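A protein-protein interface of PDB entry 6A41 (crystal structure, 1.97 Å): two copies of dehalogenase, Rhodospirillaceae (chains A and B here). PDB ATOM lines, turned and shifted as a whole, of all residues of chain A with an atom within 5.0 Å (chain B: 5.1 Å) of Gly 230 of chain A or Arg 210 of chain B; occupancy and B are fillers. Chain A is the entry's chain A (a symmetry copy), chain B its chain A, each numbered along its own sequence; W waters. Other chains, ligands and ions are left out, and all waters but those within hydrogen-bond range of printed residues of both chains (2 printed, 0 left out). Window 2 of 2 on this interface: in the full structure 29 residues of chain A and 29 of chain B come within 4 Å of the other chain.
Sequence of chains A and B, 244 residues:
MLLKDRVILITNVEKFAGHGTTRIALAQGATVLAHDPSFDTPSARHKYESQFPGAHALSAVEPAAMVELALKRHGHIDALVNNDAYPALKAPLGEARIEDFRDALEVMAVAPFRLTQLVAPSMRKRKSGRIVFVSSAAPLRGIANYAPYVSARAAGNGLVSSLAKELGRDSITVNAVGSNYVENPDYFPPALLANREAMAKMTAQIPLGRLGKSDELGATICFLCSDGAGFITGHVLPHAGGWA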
ATOM      1  N   ARG A 130      -7.428 -24.945  -5.297  1.00  0.00           N
ATOM      2  CA  ARG A 130      -6.462 -25.146  -6.327  1.00  0.00           C
ATOM      3  C   ARG A 130      -6.774 -24.161  -7.445  1.00  0.00           C
ATOM      4  O   ARG A 130      -7.941 -24.026  -7.861  1.00  0.00           O
ATOM      5  CB  ARG A 130      -6.555 -26.549  -6.921  1.00  0.00           C
ATOM      6  CG  ARG A 130      -6.334 -27.652  -5.974  1.00  0.00           C
ATOM      7  CD  ARG A 130      -4.851 -27.849  -5.859  1.00  0.00           C
ATOM      8  NE  ARG A 130      -4.567 -29.001  -5.015  1.00  0.00           N
ATOM      9  CZ  ARG A 130      -4.606 -29.043  -3.711  1.00  0.00           C
ATOM     10  NH1 ARG A 130      -4.837 -27.971  -2.959  1.00  0.00           N
ATOM     11  NH2 ARG A 130      -4.308 -30.149  -3.117  1.00  0.00           N
ATOM     12  N   THR A 173      -3.267 -23.784  -3.534  1.00  0.00           N
ATOM     13  CA  THR A 173      -2.090 -23.765  -4.437  1.00  0.00           C
ATOM     14  C   THR A 173      -2.428 -23.064  -5.757  1.00  0.00           C
ATOM     15  O   THR A 173      -3.572 -23.021  -6.166  1.00  0.00           O
ATOM     16  CB  THR A 173      -1.538 -25.166  -4.762  1.00  0.00           C
ATOM     17  OG1 THR A 173      -2.444 -25.883  -5.610  1.00  0.00           O
ATOM     18  CG2 THR A 173      -1.237 -25.955  -3.504  1.00  0.00           C
ATOM     19  N   SER A 226      -5.510 -32.256  -7.661  1.00  0.00           N
ATOM     20  CA  SER A 226      -5.701 -33.337  -6.705  1.00  0.00           C
ATOM     21  C   SER A 226      -5.070 -33.004  -5.378  1.00  0.00           C
ATOM     22  O   SER A 226      -4.130 -32.096  -5.230  1.00  0.00           O
ATOM     23  CB  SER A 226      -5.126 -34.730  -7.231  1.00  0.00           C
ATOM     24  OG  SER A 226      -3.659 -34.721  -7.165  1.00  0.00           O
ATOM     25  N   ASP A 227      -5.499 -33.781  -4.413  1.00  0.00           N
ATOM     26  CA  ASP A 227      -4.904 -33.678  -3.050  1.00  0.00           C
ATOM     27  C   ASP A 227      -3.434 -34.044  -3.007  1.00  0.00           C
ATOM     28  O   ASP A 227      -2.672 -33.433  -2.295  1.00  0.00           O
ATOM     29  CB  ASP A 227      -5.658 -34.538  -2.074  1.00  0.00           C
ATOM     30  CG  ASP A 227      -6.940 -33.958  -1.725  1.00  0.00           C
ATOM     31  OD1 ASP A 227      -7.390 -32.870  -2.214  1.00  0.00           O
ATOM     32  OD2 ASP A 227      -7.622 -34.675  -0.984  1.00  0.00           O
ATOM     33  N   GLY A 228      -3.029 -34.987  -3.872  1.00  0.00           N
ATOM     34  CA  GLY A 228      -1.679 -35.405  -3.924  1.00  0.00           C
ATOM     35  C   GLY A 228      -0.710 -34.315  -4.403  1.00  0.00           C
ATOM     36  O   GLY A 228       0.477 -34.392  -4.081  1.00  0.00           O
ATOM     37  N   ALA A 229      -1.189 -33.268  -5.099  1.00  0.00           N
ATOM     38  CA  ALA A 229      -0.358 -32.142  -5.531  1.00  0.00           C
ATOM     39  C   ALA A 229      -0.377 -30.940  -4.589  1.00  0.00           C
ATOM     40  O   ALA A 229       0.048 -29.833  -4.953  1.00  0.00           O
ATOM     41  CB  ALA A 229      -0.784 -31.691  -6.902  1.00  0.00           C
ATOM     42  N   GLY A 230      -0.768 -31.208  -3.361  1.00  0.00           N
ATOM     43  CA  GLY A 230      -0.939 -30.119  -2.368  1.00  0.00           C
ATOM     44  C   GLY A 230       0.331 -29.441  -1.905  1.00  0.00           C
ATOM     45  O   GLY A 230       0.197 -28.429  -1.233  1.00  0.00           O
ATOM     46  N   PHE A 231       1.509 -29.968  -2.216  1.00  0.00           N
ATOM     47  CA  PHE A 231       2.735 -29.326  -1.824  1.00  0.00           C
ATOM     48  C   PHE A 231       3.431 -28.691  -3.075  1.00  0.00           C
ATOM     49  O   PHE A 231       4.591 -28.269  -2.986  1.00  0.00           O
ATOM     50  CB  PHE A 231       3.663 -30.284  -1.069  1.00  0.00           C
ATOM     51  CG  PHE A 231       4.566 -29.606  -0.082  1.00  0.00           C
ATOM     52  CD1 PHE A 231       4.038 -28.765   0.879  1.00  0.00           C
ATOM     53  CD2 PHE A 231       5.968 -29.750  -0.117  1.00  0.00           C
ATOM     54  CE1 PHE A 231       4.852 -28.100   1.848  1.00  0.00           C
ATOM     55  CE2 PHE A 231       6.777 -29.102   0.821  1.00  0.00           C
ATOM     56  CZ  PHE A 231       6.245 -28.283   1.765  1.00  0.00           C
ATOM     57  N   ILE A 232       2.767 -28.706  -4.224  1.00  0.00           N
ATOM     58  CA  ILE A 232       3.284 -28.070  -5.382  1.00  0.00           C
ATOM     59  C   ILE A 232       2.562 -26.722  -5.523  1.00  0.00           C
ATOM     60  O   ILE A 232       1.326 -26.687  -5.595  1.00  0.00           O
ATOM     61  CB  ILE A 232       3.015 -28.889  -6.655  1.00  0.00           C
ATOM     62  CG1 ILE A 232       3.696 -30.241  -6.475  1.00  0.00           C
ATOM     63  CG2 ILE A 232       3.417 -28.126  -7.906  1.00  0.00           C
ATOM     64  CD1 ILE A 232       3.332 -31.268  -7.559  1.00  0.00           C
ATOM     65  N   TYR B 181      11.697 -29.654   2.207  1.00  0.00           N
ATOM     66  CA  TYR B 181      10.789 -29.500   3.312  1.00  0.00           C
ATOM     67  C   TYR B 181       9.704 -30.563   3.356  1.00  0.00           C
ATOM     68  O   TYR B 181       8.583 -30.205   3.753  1.00  0.00           O
ATOM     69  CB  TYR B 181      10.175 -28.061   3.305  1.00  0.00           C
ATOM     70  CG  TYR B 181      11.258 -27.050   3.482  1.00  0.00           C
ATOM     71  CD1 TYR B 181      11.840 -26.930   4.699  1.00  0.00           C
ATOM     72  CD2 TYR B 181      11.687 -26.223   2.469  1.00  0.00           C
ATOM     73  CE1 TYR B 181      12.859 -26.063   4.940  1.00  0.00           C
ATOM     74  CE2 TYR B 181      12.721 -25.347   2.652  1.00  0.00           C
ATOM     75  CZ  TYR B 181      13.312 -25.228   3.920  1.00  0.00           C
ATOM     76  OH  TYR B 181      14.410 -24.384   4.179  1.00  0.00           O
ATOM     77  N   THR B 203       8.946 -23.090   8.686  1.00  0.00           N
ATOM     78  CA  THR B 203       7.663 -22.833   8.067  1.00  0.00           C
ATOM     79  C   THR B 203       7.409 -21.399   7.771  1.00  0.00           C
ATOM     80  O   THR B 203       6.686 -21.100   6.839  1.00  0.00           O
ATOM     81  CB  THR B 203       6.545 -23.410   8.903  1.00  0.00           C
ATOM     82  OG1 THR B 203       6.556 -22.838  10.193  1.00  0.00           O
ATOM     83  CG2 THR B 203       6.719 -24.942   8.966  1.00  0.00           C
ATOM     84  N   ILE B 206       8.435 -21.008   4.032  1.00  0.00           N
ATOM     85  CA  ILE B 206       7.710 -21.788   3.025  1.00  0.00           C
ATOM     86  C   ILE B 206       6.365 -21.127   2.703  1.00  0.00           C
ATOM     87  O   ILE B 206       5.567 -20.960   3.631  1.00  0.00           O
ATOM     88  CB  ILE B 206       7.449 -23.166   3.572  1.00  0.00           C
ATOM     89  CG1 ILE B 206       8.763 -23.877   3.953  1.00  0.00           C
ATOM     90  CG2 ILE B 206       6.673 -24.037   2.599  1.00  0.00           C
ATOM     91  CD1 ILE B 206       8.557 -25.135   4.773  1.00  0.00           C
ATOM     92  N   LEU B 208       3.493 -22.221   1.698  1.00  0.00           N
ATOM     93  CA  LEU B 208       2.341 -22.879   2.222  1.00  0.00           C
ATOM     94  C   LEU B 208       2.363 -22.956   3.735  1.00  0.00           C
ATOM     95  O   LEU B 208       1.464 -23.440   4.324  1.00  0.00           O
ATOM     96  CB  LEU B 208       2.285 -24.281   1.653  1.00  0.00           C
ATOM     97  CG  LEU B 208       1.828 -24.333   0.183  1.00  0.00           C
ATOM     98  CD1 LEU B 208       1.809 -25.791  -0.190  1.00  0.00           C
ATOM     99  CD2 LEU B 208       0.475 -23.735  -0.067  1.00  0.00           C
ATOM    100  N   GLY B 209       3.436 -22.580   4.349  1.00  0.00           N
ATOM    101  CA  GLY B 209       3.482 -22.426   5.823  1.00  0.00           C
ATOM    102  C   GLY B 209       3.489 -23.740   6.575  1.00  0.00           C
ATOM    103  O   GLY B 209       3.154 -23.751   7.758  1.00  0.00           O
ATOM    104  N   ARG B 210       3.963 -24.826   5.960  1.00  0.00           N
ATOM    105  CA  ARG B 210       3.967 -26.144   6.569  1.00  0.00           C
ATOM    106  C   ARG B 210       4.978 -27.034   5.842  1.00  0.00           C
ATOM    107  O   ARG B 210       5.342 -26.714   4.722  1.00  0.00           O
ATOM    108  CB  ARG B 210       2.556 -26.796   6.522  1.00  0.00           C
ATOM    109  CG  ARG B 210       2.188 -27.189   5.060  1.00  0.00           C
ATOM    110  CD  ARG B 210       0.957 -28.018   4.981  1.00  0.00           C
ATOM    111  NE  ARG B 210       0.537 -28.298   3.609  1.00  0.00           N
ATOM    112  CZ  ARG B 210       0.845 -29.345   2.892  1.00  0.00           C
ATOM    113  NH1 ARG B 210       1.667 -30.367   3.301  1.00  0.00           N
ATOM    114  NH2 ARG B 210       0.302 -29.363   1.692  1.00  0.00           N
ATOM    115  N   LEU B 211       5.399 -28.151   6.453  1.00  0.00           N
ATOM    116  CA  LEU B 211       6.143 -29.192   5.738  1.00  0.00           C
ATOM    117  C   LEU B 211       5.259 -30.086   4.951  1.00  0.00           C
ATOM    118  O   LEU B 211       4.055 -30.202   5.213  1.00  0.00           O
ATOM    119  CB  LEU B 211       6.975 -30.058   6.686  1.00  0.00           C
ATOM    120  CG  LEU B 211       8.005 -29.417   7.528  1.00  0.00           C
ATOM    121  CD1 LEU B 211       8.964 -30.451   8.136  1.00  0.00           C
ATOM    122  CD2 LEU B 211       8.850 -28.381   6.898  1.00  0.00           C
ATOM    123  N   GLY B 212       5.823 -30.686   3.916  1.00  0.00           N
ATOM    124  CA  GLY B 212       5.103 -31.550   3.067  1.00  0.00           C
ATOM    125  C   GLY B 212       5.075 -32.940   3.618  1.00  0.00           C
ATOM    126  O   GLY B 212       5.828 -33.325   4.537  1.00  0.00           O
ATOM    127  N   LYS B 213       4.086 -33.677   3.165  1.00  0.00           N
ATOM    128  CA  LYS B 213       3.877 -35.055   3.543  1.00  0.00           C
ATOM    129  C   LYS B 213       4.577 -36.024   2.627  1.00  0.00           C
ATOM    130  O   LYS B 213       4.682 -35.806   1.386  1.00  0.00           O
ATOM    131  CB  LYS B 213       2.370 -35.369   3.547  1.00  0.00           C
ATOM    132  CG  LYS B 213       1.731 -34.550   4.662  1.00  0.00           C
ATOM    133  CD  LYS B 213       0.316 -34.972   4.916  1.00  0.00           C
ATOM    134  CE  LYS B 213      -0.536 -34.992   3.647  1.00  0.00           C
ATOM    135  NZ  LYS B 213      -1.944 -34.536   4.006  1.00  0.00           N
ATOM    136  N   GLU B 216       2.532 -36.847  -0.303  1.00  0.00           N
ATOM    137  CA  GLU B 216       2.486 -35.812  -1.344  1.00  0.00           C
ATOM    138  C   GLU B 216       3.645 -35.998  -2.304  1.00  0.00           C
ATOM    139  O   GLU B 216       3.454 -35.973  -3.550  1.00  0.00           O
ATOM    140  CB  GLU B 216       2.505 -34.363  -0.797  1.00  0.00           C
ATOM    141  CG  GLU B 216       1.202 -33.978  -0.167  1.00  0.00           C
ATOM    142  CD  GLU B 216       1.229 -32.751   0.798  1.00  0.00           C
ATOM    143  OE1 GLU B 216       2.225 -32.468   1.466  1.00  0.00           O
ATOM    144  OE2 GLU B 216       0.171 -32.086   0.845  1.00  0.00           O
HETATM  145  O   HOH W   1      -2.205 -32.809   0.303  1.00  0.00           O
HETATM  146  O   HOH W   2      -1.739 -27.317   0.100  1.00  0.00           O
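The backbone carbonyl oxygen of Gly 230 of chain A is in hydrogen-bond range of the guanidinium group of Arg 210 of chain B (3.1 Å). The backbone carbonyl oxygen (O) of Glu 216 of chain B lies close to the backbone carbonyl oxygen (O) of Gly 228 of chain A, at 3.4 Å.
O of Tyr 181 of chain B lies within hydrogen-bond range of N of Gly 212 of chain B, 2.8 Å away. NH1 of Arg 210 of chain B is in salt-bridge range of OE1 of Glu 216 of chain B (2.8 Å). The side-chain carboxylate (OE1) of Glu 216 of chain B sits at hydrogen-bond distance from the backbone NH (N) of Lys 213 of chain B (2.8 Å). N of Gly 228 of chain A lies close to OG of Ser 226 of chain A, 3.4 Å away.
Among the printed residues, merely in contact across the chains: Phe 231 of chain A with Arg 210 of chain B (3.2 Å), Phe 231 of chain A with Gly 212 of chain B (3.3 Å), Gly 230 of chain A with Leu 208 of chain B (3.3 Å), Phe 231 of chain A with Tyr 181 of chain B (3.6 Å), Phe 231 of chain A with Glu 216 of chain B (3.6 Å), Phe 231 of chain A with Leu 211 of chain B (3.7 Å), Gly 230 of chain A with Glu 216 of chain B (3.8 Å) and Phe 231 of chain A with Leu 208 of chain B (3.9 Å).
Arg 130 of chain A touches none of the printed residues of chain B. Ser 226 of chain A touches none of the printed residues of chain B. Of the printed residues of chain B, Gly 228 of chain A touches Glu 216 (3.4 Å). Gly 230 of chain A touches three residues of chain B. Printed residues of chain A within 4 Å of Tyr 181 of chain B: Phe 231 (3.6 Å). Of the printed residues of chain A, Leu 208 of chain B touches Gly 230 (3.3 Å) and Phe 231 (3.9 Å). Arg 210 of chain B touches just these residues of chain A: Gly 230 (3.1 Å) and Phe 231 (3.2 Å). Printed residues of chain A within 4 Å of Leu 211 of chain B: Phe 231 (3.7 Å). Of the printed residues of chain A, Glu 216 of chain B touches Gly 228, Gly 230 and Phe 231. The nearest printed residue of chain B that does not touch Gly 230 of chain A is Gly 212 of chain B (7.2 Å). The nearest printed residue of chain A that does not touch Arg 210 of chain B is Thr 173 of chain A (6.4 Å). The nearest printed residue of chain A that does not touch Glu 216 of chain B is Asp 227 of chain A (4.4 Å).
Hydrophobic or aromatic side chains of chain B that line the printed part of chain A: Leu 208. Among the printed residues, no Asp or Glu carboxylate lies within 4 Å of a Lys or Arg side-chain nitrogen of the other chain.
No position is printed for both chains. Of the 10 pairs that touch across the chains among the printed residues, none has its exchanged pair printed and touching as well.
Water W1 lies within hydrogen-bond range of OE2 of Glu 216 of chain B (2.5 Å) and O of Asp 227 of chain A (2.7 Å). Water W2 lies within hydrogen-bond range of O of Gly 230 of chain A (2.6 Å) and NH2 of Arg 210 of chain B (3.3 Å).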
